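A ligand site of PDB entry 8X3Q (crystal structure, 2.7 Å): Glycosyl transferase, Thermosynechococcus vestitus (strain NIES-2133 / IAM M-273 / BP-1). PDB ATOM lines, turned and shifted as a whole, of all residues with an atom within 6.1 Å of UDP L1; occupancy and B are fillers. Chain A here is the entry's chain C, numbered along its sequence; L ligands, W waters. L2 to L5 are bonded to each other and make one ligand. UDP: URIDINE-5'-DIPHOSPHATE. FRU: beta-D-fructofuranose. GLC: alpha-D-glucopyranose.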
ATOM      1  N   PRO A  19     -34.888 -21.701  11.335  1.00  0.00           N
ATOM      2  CA  PRO A  19     -36.068 -21.362  10.531  1.00  0.00           C
ATOM      3  C   PRO A  19     -35.801 -21.435   9.041  1.00  0.00           C
ATOM      4  O   PRO A  19     -36.694 -21.819   8.269  1.00  0.00           O
ATOM      5  CB  PRO A  19     -36.410 -19.937  10.976  1.00  0.00           C
ATOM      6  CG  PRO A  19     -35.106 -19.392  11.490  1.00  0.00           C
ATOM      7  CD  PRO A  19     -34.403 -20.557  12.124  1.00  0.00           C
ATOM      8  N   ALA A  20     -34.601 -21.076   8.595  1.00  0.00           N
ATOM      9  CA  ALA A  20     -34.259 -21.115   7.176  1.00  0.00           C
ATOM     10  C   ALA A  20     -32.947 -21.859   6.957  1.00  0.00           C
ATOM     11  O   ALA A  20     -32.861 -23.059   7.239  1.00  0.00           O
ATOM     12  CB  ALA A  20     -34.183 -19.701   6.609  1.00  0.00           C
ATOM     13  N   TYR A  21     -31.925 -21.164   6.462  1.00  0.00           N
ATOM     14  CA  TYR A  21     -30.653 -21.818   6.192  1.00  0.00           C
ATOM     15  C   TYR A  21     -30.041 -22.366   7.473  1.00  0.00           C
ATOM     16  O   TYR A  21     -30.153 -21.771   8.546  1.00  0.00           O
ATOM     17  CB  TYR A  21     -29.668 -20.845   5.535  1.00  0.00           C
ATOM     18  CG  TYR A  21     -28.311 -21.465   5.274  1.00  0.00           C
ATOM     19  CD1 TYR A  21     -28.081 -22.224   4.137  1.00  0.00           C
ATOM     20  CD2 TYR A  21     -27.274 -21.317   6.189  1.00  0.00           C
ATOM     21  CE1 TYR A  21     -26.857 -22.811   3.907  1.00  0.00           C
ATOM     22  CE2 TYR A  21     -26.043 -21.905   5.965  1.00  0.00           C
ATOM     23  CZ  TYR A  21     -25.836 -22.648   4.828  1.00  0.00           C
ATOM     24  OH  TYR A  21     -24.616 -23.227   4.604  1.00  0.00           O
ATOM     25  N   GLY A  22     -29.392 -23.522   7.360  1.00  0.00           N
ATOM     26  CA  GLY A  22     -28.703 -24.136   8.480  1.00  0.00           C
ATOM     27  C   GLY A  22     -28.627 -25.639   8.361  1.00  0.00           C
ATOM     28  O   GLY A  22     -29.636 -26.333   8.504  1.00  0.00           O
ATOM     29  N   GLY A  23     -27.436 -26.150   8.087  1.00  0.00           N
ATOM     30  CA  GLY A  23     -27.245 -27.577   7.927  1.00  0.00           C
ATOM     31  C   GLY A  23     -26.836 -28.291   9.204  1.00  0.00           C
ATOM     32  O   GLY A  23     -27.555 -29.183   9.668  1.00  0.00           O
ATOM     33  N   VAL A  24     -25.704 -27.902   9.774  1.00  0.00           N
ATOM     34  CA  VAL A  24     -25.190 -28.567  10.968  1.00  0.00           C
ATOM     35  C   VAL A  24     -26.187 -28.443  12.118  1.00  0.00           C
ATOM     36  O   VAL A  24     -26.456 -29.416  12.840  1.00  0.00           O
ATOM     37  CB  VAL A  24     -23.819 -27.990  11.364  1.00  0.00           C
ATOM     38  CG1 VAL A  24     -23.323 -28.641  12.651  1.00  0.00           C
ATOM     39  CG2 VAL A  24     -22.829 -28.185  10.230  1.00  0.00           C
ATOM     40  N   LEU A  26     -29.404 -28.138  12.005  1.00  0.00           N
ATOM     41  CA  LEU A  26     -30.554 -29.002  11.776  1.00  0.00           C
ATOM     42  C   LEU A  26     -30.271 -30.437  12.197  1.00  0.00           C
ATOM     43  O   LEU A  26     -31.112 -31.081  12.842  1.00  0.00           O
ATOM     44  CB  LEU A  26     -30.959 -28.937  10.300  1.00  0.00           C
ATOM     45  CG  LEU A  26     -31.936 -30.001   9.777  1.00  0.00           C
ATOM     46  CD1 LEU A  26     -33.308 -29.815  10.380  1.00  0.00           C
ATOM     47  CD2 LEU A  26     -31.995 -29.972   8.251  1.00  0.00           C
ATOM     48  N   ILE A 160     -32.718 -36.439   7.630  1.00  0.00           N
ATOM     49  CA  ILE A 160     -33.776 -35.447   7.780  1.00  0.00           C
ATOM     50  C   ILE A 160     -35.006 -36.153   8.350  1.00  0.00           C
ATOM     51  O   ILE A 160     -35.042 -37.382   8.472  1.00  0.00           O
ATOM     52  CB  ILE A 160     -34.119 -34.737   6.464  1.00  0.00           C
ATOM     53  CG1 ILE A 160     -34.451 -35.753   5.370  1.00  0.00           C
ATOM     54  CG2 ILE A 160     -32.970 -33.835   6.030  1.00  0.00           C
ATOM     55  CD1 ILE A 160     -34.933 -35.131   4.077  1.00  0.00           C
ATOM     56  N   LEU A 180     -31.419 -25.024  -4.674  1.00  0.00           N
ATOM     57  CA  LEU A 180     -31.646 -24.747  -3.258  1.00  0.00           C
ATOM     58  C   LEU A 180     -30.318 -24.827  -2.549  1.00  0.00           C
ATOM     59  O   LEU A 180     -29.648 -25.866  -2.589  1.00  0.00           O
ATOM     60  CB  LEU A 180     -32.644 -25.738  -2.654  1.00  0.00           C
ATOM     61  CG  LEU A 180     -32.742 -25.682  -1.124  1.00  0.00           C
ATOM     62  CD1 LEU A 180     -33.124 -24.289  -0.647  1.00  0.00           C
ATOM     63  CD2 LEU A 180     -33.733 -26.714  -0.601  1.00  0.00           C
ATOM     64  N   GLY A 181     -29.937 -23.748  -1.897  1.00  0.00           N
ATOM     65  CA  GLY A 181     -28.680 -23.708  -1.175  1.00  0.00           C
ATOM     66  C   GLY A 181     -28.132 -22.302  -1.135  1.00  0.00           C
ATOM     67  O   GLY A 181     -28.608 -21.391  -1.809  1.00  0.00           O
ATOM     68  N   ARG A 182     -27.088 -22.145  -0.330  1.00  0.00           N
ATOM     69  CA  ARG A 182     -26.400 -20.860  -0.242  1.00  0.00           C
ATOM     70  C   ARG A 182     -25.782 -20.505  -1.587  1.00  0.00           C
ATOM     71  O   ARG A 182     -25.285 -21.370  -2.310  1.00  0.00           O
ATOM     72  CB  ARG A 182     -25.333 -20.911   0.853  1.00  0.00           C
ATOM     73  CG  ARG A 182     -24.052 -21.568   0.387  1.00  0.00           C
ATOM     74  CD  ARG A 182     -23.189 -22.106   1.501  1.00  0.00           C
ATOM     75  NE  ARG A 182     -21.965 -22.649   0.944  1.00  0.00           N
ATOM     76  CZ  ARG A 182     -21.116 -23.423   1.607  1.00  0.00           C
ATOM     77  NH1 ARG A 182     -21.366 -23.759   2.864  1.00  0.00           N
ATOM     78  NH2 ARG A 182     -20.018 -23.862   1.014  1.00  0.00           N
ATOM     79  N   LYS A 187     -21.394 -24.364  -4.424  1.00  0.00           N
ATOM     80  CA  LYS A 187     -22.649 -24.973  -4.828  1.00  0.00           C
ATOM     81  C   LYS A 187     -22.933 -24.797  -6.317  1.00  0.00           C
ATOM     82  O   LYS A 187     -23.824 -25.457  -6.846  1.00  0.00           O
ATOM     83  CB  LYS A 187     -23.813 -24.392  -4.026  1.00  0.00           C
ATOM     84  CG  LYS A 187     -23.677 -24.569  -2.524  1.00  0.00           C
ATOM     85  CD  LYS A 187     -23.540 -26.039  -2.166  1.00  0.00           C
ATOM     86  CE  LYS A 187     -23.781 -26.274  -0.688  1.00  0.00           C
ATOM     87  NZ  LYS A 187     -23.437 -27.671  -0.294  1.00  0.00           N
ATOM     88  N   ALA A 206     -33.472 -20.712  -4.475  1.00  0.00           N
ATOM     89  CA  ALA A 206     -33.662 -20.274  -3.101  1.00  0.00           C
ATOM     90  C   ALA A 206     -32.355 -20.445  -2.343  1.00  0.00           C
ATOM     91  O   ALA A 206     -31.588 -21.374  -2.597  1.00  0.00           O
ATOM     92  CB  ALA A 206     -34.772 -21.066  -2.403  1.00  0.00           C
ATOM     93  N   GLY A 207     -32.112 -19.546  -1.415  1.00  0.00           N
ATOM     94  CA  GLY A 207     -30.929 -19.608  -0.594  1.00  0.00           C
ATOM     95  C   GLY A 207     -30.496 -18.238  -0.136  1.00  0.00           C
ATOM     96  O   GLY A 207     -30.954 -17.212  -0.633  1.00  0.00           O
ATOM     97  N   LYS A 208     -29.584 -18.230   0.824  1.00  0.00           N
ATOM     98  CA  LYS A 208     -28.991 -17.010   1.347  1.00  0.00           C
ATOM     99  C   LYS A 208     -27.762 -16.603   0.533  1.00  0.00           C
ATOM    100  O   LYS A 208     -27.119 -17.432  -0.127  1.00  0.00           O
ATOM    101  CB  LYS A 208     -28.616 -17.179   2.815  1.00  0.00           C
ATOM    102  CG  LYS A 208     -27.585 -18.279   3.071  1.00  0.00           C
ATOM    103  CD  LYS A 208     -26.725 -17.960   4.280  1.00  0.00           C
ATOM    104  CE  LYS A 208     -25.488 -18.831   4.310  1.00  0.00           C
ATOM    105  NZ  LYS A 208     -24.663 -18.588   5.539  1.00  0.00           N
ATOM    106  N   GLY A 234     -34.576 -15.912  -2.473  1.00  0.00           N
ATOM    107  CA  GLY A 234     -33.769 -15.694  -1.291  1.00  0.00           C
ATOM    108  C   GLY A 234     -33.963 -16.789  -0.252  1.00  0.00           C
ATOM    109  O   GLY A 234     -34.468 -17.879  -0.556  1.00  0.00           O
ATOM    110  N   GLU A 235     -33.544 -16.494   0.973  1.00  0.00           N
ATOM    111  CA  GLU A 235     -33.581 -17.476   2.053  1.00  0.00           C
ATOM    112  C   GLU A 235     -34.998 -17.987   2.282  1.00  0.00           C
ATOM    113  O   GLU A 235     -35.913 -17.195   2.564  1.00  0.00           O
ATOM    114  CB  GLU A 235     -33.020 -16.869   3.335  1.00  0.00           C
ATOM    115  CG  GLU A 235     -32.282 -17.859   4.216  1.00  0.00           C
ATOM    116  CD  GLU A 235     -31.654 -17.207   5.432  1.00  0.00           C
ATOM    117  OE1 GLU A 235     -31.287 -16.023   5.347  1.00  0.00           O
ATOM    118  OE2 GLU A 235     -31.536 -17.883   6.483  1.00  0.00           O
ATOM    119  N   ALA A 236     -35.178 -19.289   2.167  1.00  0.00           N
ATOM    120  CA  ALA A 236     -36.488 -19.921   2.286  1.00  0.00           C
ATOM    121  C   ALA A 236     -36.579 -20.719   3.583  1.00  0.00           C
ATOM    122  O   ALA A 236     -35.600 -21.335   4.011  1.00  0.00           O
ATOM    123  CB  ALA A 236     -36.759 -20.840   1.091  1.00  0.00           C
ATOM    124  N   ASP A 237     -37.752 -20.693   4.199  1.00  0.00           N
ATOM    125  CA  ASP A 237     -38.024 -21.528   5.363  1.00  0.00           C
ATOM    126  C   ASP A 237     -38.430 -22.922   4.917  1.00  0.00           C
ATOM    127  O   ASP A 237     -38.450 -23.239   3.725  1.00  0.00           O
ATOM    128  CB  ASP A 237     -39.065 -20.868   6.264  1.00  0.00           C
ATOM    129  CG  ASP A 237     -40.461 -20.870   5.649  1.00  0.00           C
ATOM    130  OD1 ASP A 237     -40.583 -21.013   4.418  1.00  0.00           O
ATOM    131  OD2 ASP A 237     -41.440 -20.702   6.413  1.00  0.00           O
ATOM    132  N   HIS A 238     -38.757 -23.791   5.883  1.00  0.00           N
ATOM    133  CA  HIS A 238     -39.070 -25.175   5.549  1.00  0.00           C
ATOM    134  C   HIS A 238     -40.249 -25.315   4.590  1.00  0.00           C
ATOM    135  O   HIS A 238     -40.114 -26.048   3.601  1.00  0.00           O
ATOM    136  CB  HIS A 238     -39.290 -25.996   6.830  1.00  0.00           C
ATOM    137  CG  HIS A 238     -39.738 -27.398   6.573  1.00  0.00           C
ATOM    138  ND1 HIS A 238     -38.846 -28.431   6.337  1.00  0.00           N
ATOM    139  CD2 HIS A 238     -40.974 -27.939   6.488  1.00  0.00           C
ATOM    140  CE1 HIS A 238     -39.523 -29.544   6.126  1.00  0.00           C
ATOM    141  NE2 HIS A 238     -40.813 -29.275   6.214  1.00  0.00           N
ATOM    142  N   LYS A 241     -39.082 -24.057   0.883  1.00  0.00           N
ATOM    143  CA  LYS A 241     -38.138 -24.926   0.166  1.00  0.00           C
ATOM    144  C   LYS A 241     -38.803 -26.234  -0.256  1.00  0.00           C
ATOM    145  O   LYS A 241     -38.406 -26.827  -1.259  1.00  0.00           O
ATOM    146  CB  LYS A 241     -36.908 -25.192   1.030  1.00  0.00           C
ATOM    147  CG  LYS A 241     -37.081 -26.282   2.076  1.00  0.00           C
ATOM    148  CD  LYS A 241     -35.957 -26.230   3.094  1.00  0.00           C
ATOM    149  CE  LYS A 241     -36.041 -27.404   4.059  1.00  0.00           C
ATOM    150  NZ  LYS A 241     -34.916 -27.401   5.036  1.00  0.00           N
ATOM    151  N   PHE A 253     -27.720 -29.852  -8.590  1.00  0.00           N
ATOM    152  CA  PHE A 253     -26.724 -29.833  -7.523  1.00  0.00           C
ATOM    153  C   PHE A 253     -25.328 -29.850  -8.151  1.00  0.00           C
ATOM    154  O   PHE A 253     -24.564 -30.789  -7.967  1.00  0.00           O
ATOM    155  CB  PHE A 253     -26.927 -31.017  -6.584  1.00  0.00           C
ATOM    156  CG  PHE A 253     -26.187 -30.916  -5.280  1.00  0.00           C
ATOM    157  CD1 PHE A 253     -26.548 -29.977  -4.327  1.00  0.00           C
ATOM    158  CD2 PHE A 253     -25.135 -31.777  -5.000  1.00  0.00           C
ATOM    159  CE1 PHE A 253     -25.868 -29.890  -3.129  1.00  0.00           C
ATOM    160  CE2 PHE A 253     -24.460 -31.697  -3.796  1.00  0.00           C
ATOM    161  CZ  PHE A 253     -24.821 -30.758  -2.860  1.00  0.00           C
ATOM    162  N   TRP A 257     -16.989 -28.555  -5.672  1.00  0.00           N
ATOM    163  CA  TRP A 257     -16.486 -28.520  -4.312  1.00  0.00           C
ATOM    164  C   TRP A 257     -16.497 -29.940  -3.732  1.00  0.00           C
ATOM    165  O   TRP A 257     -17.301 -30.781  -4.136  1.00  0.00           O
ATOM    166  CB  TRP A 257     -17.359 -27.560  -3.493  1.00  0.00           C
ATOM    167  CG  TRP A 257     -17.161 -27.515  -2.026  1.00  0.00           C
ATOM    168  CD1 TRP A 257     -15.985 -27.346  -1.361  1.00  0.00           C
ATOM    169  CD2 TRP A 257     -18.181 -27.598  -1.026  1.00  0.00           C
ATOM    170  NE1 TRP A 257     -16.217 -27.323  -0.009  1.00  0.00           N
ATOM    171  CE2 TRP A 257     -17.553 -27.486   0.229  1.00  0.00           C
ATOM    172  CE3 TRP A 257     -19.568 -27.764  -1.072  1.00  0.00           C
ATOM    173  CZ2 TRP A 257     -18.263 -27.530   1.423  1.00  0.00           C
ATOM    174  CZ3 TRP A 257     -20.266 -27.816   0.122  1.00  0.00           C
ATOM    175  CH2 TRP A 257     -19.617 -27.698   1.349  1.00  0.00           C
ATOM    176  N   GLU A 259     -17.819 -31.736  -1.537  1.00  0.00           N
ATOM    177  CA  GLU A 259     -18.992 -31.731  -0.672  1.00  0.00           C
ATOM    178  C   GLU A 259     -18.890 -32.810   0.392  1.00  0.00           C
ATOM    179  O   GLU A 259     -18.718 -33.996   0.058  1.00  0.00           O
ATOM    180  CB  GLU A 259     -20.260 -31.924  -1.501  1.00  0.00           C
ATOM    181  CG  GLU A 259     -21.544 -31.978  -0.681  1.00  0.00           C
ATOM    182  CD  GLU A 259     -22.017 -30.605  -0.236  1.00  0.00           C
ATOM    183  OE1 GLU A 259     -22.412 -29.802  -1.118  1.00  0.00           O
ATOM    184  OE2 GLU A 259     -21.994 -30.331   0.979  1.00  0.00           O
ATOM    185  N   PRO A 260     -19.001 -32.470   1.680  1.00  0.00           N
ATOM    186  CA  PRO A 260     -18.973 -33.521   2.714  1.00  0.00           C
ATOM    187  C   PRO A 260     -20.224 -34.389   2.719  1.00  0.00           C
ATOM    188  O   PRO A 260     -20.117 -35.597   2.955  1.00  0.00           O
ATOM    189  CB  PRO A 260     -18.827 -32.728   4.024  1.00  0.00           C
ATOM    190  CG  PRO A 260     -18.445 -31.332   3.615  1.00  0.00           C
ATOM    191  CD  PRO A 260     -19.041 -31.117   2.264  1.00  0.00           C
ATOM    192  N   PHE A 261     -21.391 -33.803   2.471  1.00  0.00           N
ATOM    193  CA  PHE A 261     -22.631 -34.570   2.392  1.00  0.00           C
ATOM    194  C   PHE A 261     -23.589 -33.907   1.423  1.00  0.00           C
ATOM    195  O   PHE A 261     -23.623 -34.279   0.241  1.00  0.00           O
ATOM    196  CB  PHE A 261     -23.271 -34.697   3.782  1.00  0.00           C
ATOM    197  CG  PHE A 261     -24.381 -35.721   3.845  1.00  0.00           C
ATOM    198  CD1 PHE A 261     -25.637 -35.461   3.333  1.00  0.00           C
ATOM    199  CD2 PHE A 261     -24.155 -36.963   4.436  1.00  0.00           C
ATOM    200  CE1 PHE A 261     -26.646 -36.402   3.389  1.00  0.00           C
ATOM    201  CE2 PHE A 261     -25.169 -37.911   4.497  1.00  0.00           C
ATOM    202  CZ  PHE A 261     -26.413 -37.623   3.974  1.00  0.00           C
ATOM    203  N   GLY A 262     -24.362 -32.933   1.892  1.00  0.00           N
ATOM    204  CA  GLY A 262     -25.320 -32.244   1.045  1.00  0.00           C
ATOM    205  C   GLY A 262     -26.759 -32.551   1.416  1.00  0.00           C
ATOM    206  O   GLY A 262     -27.416 -33.371   0.768  1.00  0.00           O
ATOM    207  N   LEU A 263     -27.265 -31.878   2.457  1.00  0.00           N
ATOM    208  CA  LEU A 263     -28.598 -32.190   2.970  1.00  0.00           C
ATOM    209  C   LEU A 263     -29.698 -31.840   1.978  1.00  0.00           C
ATOM    210  O   LEU A 263     -30.767 -32.462   1.994  1.00  0.00           O
ATOM    211  CB  LEU A 263     -28.831 -31.471   4.291  1.00  0.00           C
ATOM    212  CG  LEU A 263     -28.109 -32.048   5.505  1.00  0.00           C
ATOM    213  CD1 LEU A 263     -27.819 -30.956   6.530  1.00  0.00           C
ATOM    214  CD2 LEU A 263     -28.934 -33.162   6.128  1.00  0.00           C
ATOM    215  N   VAL A 264     -29.474 -30.858   1.099  1.00  0.00           N
ATOM    216  CA  VAL A 264     -30.495 -30.481   0.139  1.00  0.00           C
ATOM    217  C   VAL A 264     -30.772 -31.603  -0.858  1.00  0.00           C
ATOM    218  O   VAL A 264     -31.854 -31.626  -1.477  1.00  0.00           O
ATOM    219  CB  VAL A 264     -30.106 -29.190  -0.613  1.00  0.00           C
ATOM    220  CG1 VAL A 264     -29.976 -28.033   0.369  1.00  0.00           C
ATOM    221  CG2 VAL A 264     -28.814 -29.393  -1.381  1.00  0.00           C
ATOM    222  N   MET A 265     -29.840 -32.541  -1.034  1.00  0.00           N
ATOM    223  CA  MET A 265     -30.083 -33.662  -1.926  1.00  0.00           C
ATOM    224  C   MET A 265     -31.159 -34.581  -1.374  1.00  0.00           C
ATOM    225  O   MET A 265     -32.153 -34.873  -2.048  1.00  0.00           O
ATOM    226  CB  MET A 265     -28.778 -34.440  -2.158  1.00  0.00           C
ATOM    227  CG  MET A 265     -27.825 -33.777  -3.134  1.00  0.00           C
ATOM    228  SD  MET A 265     -26.494 -34.878  -3.632  1.00  0.00           S
ATOM    229  CE  MET A 265     -25.530 -34.923  -2.129  1.00  0.00           C
ATOM    230  N   GLU A 267     -33.210 -33.836   0.922  1.00  0.00           N
ATOM    231  CA  GLU A 267     -34.435 -33.055   1.046  1.00  0.00           C
ATOM    232  C   GLU A 267     -35.189 -33.005  -0.267  1.00  0.00           C
ATOM    233  O   GLU A 267     -36.426 -32.993  -0.287  1.00  0.00           O
ATOM    234  CB  GLU A 267     -34.115 -31.647   1.543  1.00  0.00           C
ATOM    235  CG  GLU A 267     -33.611 -31.586   2.973  1.00  0.00           C
ATOM    236  CD  GLU A 267     -33.066 -30.216   3.347  1.00  0.00           C
ATOM    237  OE1 GLU A 267     -32.568 -29.521   2.445  1.00  0.00           O
ATOM    238  OE2 GLU A 267     -33.140 -29.849   4.537  1.00  0.00           O
HETATM  239  N1  UDP L   1     -31.551 -24.386   3.604  1.00  0.00           N
HETATM  240  C2  UDP L   1     -32.724 -23.693   3.664  1.00  0.00           C
HETATM  241  N3  UDP L   1     -32.974 -22.694   2.952  1.00  0.00           N
HETATM  242  C4  UDP L   1     -32.228 -22.200   2.110  1.00  0.00           C
HETATM  243  C5  UDP L   1     -31.037 -22.662   1.825  1.00  0.00           C
HETATM  244  C6  UDP L   1     -30.680 -23.814   2.606  1.00  0.00           C
HETATM  245  O2  UDP L   1     -33.546 -24.051   4.443  1.00  0.00           O
HETATM  246  O4  UDP L   1     -32.621 -21.256   1.514  1.00  0.00           O
HETATM  247  C1' UDP L   1     -31.253 -25.511   4.384  1.00  0.00           C
HETATM  248  C2' UDP L   1     -31.185 -26.718   3.533  1.00  0.00           C
HETATM  249  O2' UDP L   1     -32.519 -27.276   3.358  1.00  0.00           O
HETATM  250  C3' UDP L   1     -30.326 -27.636   4.245  1.00  0.00           C
HETATM  251  C4' UDP L   1     -29.319 -26.784   4.932  1.00  0.00           C
HETATM  252  O4' UDP L   1     -29.898 -25.393   5.052  1.00  0.00           O
HETATM  253  O3' UDP L   1     -31.101 -28.365   5.243  1.00  0.00           O
HETATM  254  C5' UDP L   1     -28.073 -26.734   4.146  1.00  0.00           C
HETATM  255  O5' UDP L   1     -27.374 -27.951   4.275  1.00  0.00           O
HETATM  256  PA  UDP L   1     -26.351 -28.395   3.062  1.00  0.00           P
HETATM  257  O1A UDP L   1     -25.480 -29.485   3.482  1.00  0.00           O
HETATM  258  O2A UDP L   1     -27.064 -29.007   1.949  1.00  0.00           O
HETATM  259  O3A UDP L   1     -25.498 -27.068   2.565  1.00  0.00           O
HETATM  260  PB  UDP L   1     -24.114 -26.527   3.273  1.00  0.00           P
HETATM  261  O1B UDP L   1     -22.958 -27.324   2.887  1.00  0.00           O
HETATM  262  O2B UDP L   1     -24.136 -26.746   4.729  1.00  0.00           O
HETATM  263  O3B UDP L   1     -23.880 -24.934   2.922  1.00  0.00           O
HETATM  264  C1  FRU L   2     -17.413 -23.510   3.782  1.00  0.00           C
HETATM  265  C2  FRU L   2     -16.048 -23.317   4.516  1.00  0.00           C
HETATM  266  C3  FRU L   2     -15.687 -22.081   4.345  1.00  0.00           C
HETATM  267  C4  FRU L   2     -14.243 -22.077   3.858  1.00  0.00           C
HETATM  268  C5  FRU L   2     -13.852 -23.563   3.656  1.00  0.00           C
HETATM  269  C6  FRU L   2     -12.798 -24.003   4.731  1.00  0.00           C
HETATM  270  O1  FRU L   2     -17.160 -23.798   2.431  1.00  0.00           O
HETATM  271  O2  FRU L   2     -16.074 -23.640   5.912  1.00  0.00           O
HETATM  272  O3  FRU L   2     -15.789 -21.323   5.648  1.00  0.00           O
HETATM  273  O4  FRU L   2     -14.137 -21.453   2.650  1.00  0.00           O
HETATM  274  O5  FRU L   2     -14.940 -24.236   3.774  1.00  0.00           O
HETATM  275  O6  FRU L   2     -11.941 -22.952   5.077  1.00  0.00           O
HETATM  276  C1  GLC L   3     -17.215 -24.358   6.345  1.00  0.00           C
HETATM  277  C2  GLC L   3     -17.997 -23.502   7.280  1.00  0.00           C
HETATM  278  C3  GLC L   3     -17.166 -23.078   8.391  1.00  0.00           C
HETATM  279  C4  GLC L   3     -16.507 -24.207   9.123  1.00  0.00           C
HETATM  280  C5  GLC L   3     -16.589 -25.647   8.505  1.00  0.00           C
HETATM  281  C6  GLC L   3     -17.561 -26.429   9.190  1.00  0.00           C
HETATM  282  O2  GLC L   3     -18.564 -22.365   6.441  1.00  0.00           O
HETATM  283  O3  GLC L   3     -17.938 -22.353   9.427  1.00  0.00           O
HETATM  284  O4  GLC L   3     -15.123 -23.872   9.265  1.00  0.00           O
HETATM  285  O5  GLC L   3     -16.830 -25.644   6.985  1.00  0.00           O
HETATM  286  O6  GLC L   3     -18.635 -26.702   8.323  1.00  0.00           O
HETATM  287  C1  GLC L   4     -19.602 -21.657   7.094  1.00  0.00           C
HETATM  288  C2  GLC L   4     -20.974 -22.041   6.627  1.00  0.00           C
HETATM  289  C3  GLC L   4     -21.347 -21.471   5.330  1.00  0.00           C
HETATM  290  C4  GLC L   4     -21.041 -20.019   5.215  1.00  0.00           C
HETATM  291  C5  GLC L   4     -19.547 -19.747   5.486  1.00  0.00           C
HETATM  292  C6  GLC L   4     -19.269 -18.370   5.380  1.00  0.00           C
HETATM  293  O2  GLC L   4     -21.144 -23.536   6.555  1.00  0.00           O
HETATM  294  O3  GLC L   4     -22.805 -21.641   5.144  1.00  0.00           O
HETATM  295  O4  GLC L   4     -21.386 -19.557   3.899  1.00  0.00           O
HETATM  296  O5  GLC L   4     -19.301 -20.224   6.932  1.00  0.00           O
HETATM  297  O6  GLC L   4     -17.886 -18.185   5.536  1.00  0.00           O
HETATM  298  C1  GLC L   5     -21.280 -24.153   7.837  1.00  0.00           C
HETATM  299  C2  GLC L   5     -22.044 -25.437   7.702  1.00  0.00           C
HETATM  300  C3  GLC L   5     -23.462 -25.253   7.680  1.00  0.00           C
HETATM  301  C4  GLC L   5     -23.938 -24.559   8.902  1.00  0.00           C
HETATM  302  C5  GLC L   5     -23.325 -23.133   9.025  1.00  0.00           C
HETATM  303  C6  GLC L   5     -23.593 -22.623  10.329  1.00  0.00           C
HETATM  304  O2  GLC L   5     -21.607 -26.112   6.433  1.00  0.00           O
HETATM  305  O3  GLC L   5     -24.117 -26.577   7.593  1.00  0.00           O
HETATM  306  O4  GLC L   5     -25.353 -24.432   8.867  1.00  0.00           O
HETATM  307  O5  GLC L   5     -21.806 -23.214   8.844  1.00  0.00           O
HETATM  308  O6  GLC L   5     -22.883 -23.405  11.260  1.00  0.00           O
HETATM  309  O   HOH W   1     -26.754 -24.333   0.785  1.00  0.00           O
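OE1 of Glu 267 is in hydrogen-bond range of O2' of UDP L1. The side-chain hydroxyl (OH) of Tyr 21 is in hydrogen-bond range of an oxygen (O3B) of UDP L1 (2.5 Å). The guanidinium group (NH1) of Arg 182 lies within salt-bridge range of an oxygen (O3B) of UDP L1. N of Leu 263 sits at hydrogen-bond distance from O2A of UDP L1 (2.9 Å). NZ of Lys 241 lies within hydrogen-bond range of O2' of UDP L1 (2.9 Å). The backbone NH (N) of Gly 22 is in hydrogen-bond range of an oxygen (O4') of UDP L1, at 3.0 Å. An oxygen (O4) of UDP L1 is in hydrogen-bond range of the backbone NH of Ala 236, at 3.3 Å. N3 of UDP L1 lies within hydrogen-bond range of O of Ala 236 (3.1 Å). An oxygen (O2A) of UDP L1 sits at hydrogen-bond distance from the backbone NH (N) of Val 264 (3.2 Å). The backbone NH (N) of Gly 207 sits close to an oxygen (O4) of UDP L1. The side-chain amino group (NZ) of Lys 187 lies within salt-bridge range of an oxygen (O1B) of UDP L1 (3.2 Å). O3 of GLC L4 is in hydrogen-bond range of OH of Tyr 21 (2.5 Å). An oxygen (O1) of FRU L2 sits at hydrogen-bond distance from the guanidinium group of Arg 182 (3.2 Å). N of Gly 23 lies within hydrogen-bond range of O4 of GLC L5 (2.8 Å). An oxygen (O3) of GLC L5 lies within hydrogen-bond range of the backbone NH (N) of Val 24 (3.0 Å).
Water W1 bridges the backbone NH of Arg 182 and an oxygen (O3A) of UDP L1.
NZ of Lys 241 lies within salt-bridge range of OE2 of Glu 267. The side-chain carboxylate of Glu 235 sits at hydrogen-bond distance from the backbone NH of Tyr 21 (3.3 Å). The backbone carbonyl oxygen (O) of Gly 207 sits at hydrogen-bond distance from the backbone NH (N) of Glu 235 (3.1 Å). N of Gly 207 is in hydrogen-bond range of O of Gly 234 (3.0 Å). The side-chain amino group (NZ) of Lys 187 is in salt-bridge range of the side-chain carboxylate (OE1) of Glu 259 (2.5 Å). O of Ala 206 lies within hydrogen-bond range of N of Gly 181.
O of Ala 20 sits close to O2 of UDP L1 (3.0 Å). Merely in contact with UDP L1: Leu 26 (3.5 Å), Leu 180 (3.6 Å), Gly 262 (3.6 Å), Gly 23 (3.7 Å), Glu 259 (3.7 Å), Trp 257 (3.7 Å), Glu 235 (3.9 Å), Ala 206 (3.95 Å) and Gly 181 (3.96 Å).
O2B of UDP L1 lies within hydrogen-bond range of O3 of GLC L5 (2.9 Å).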
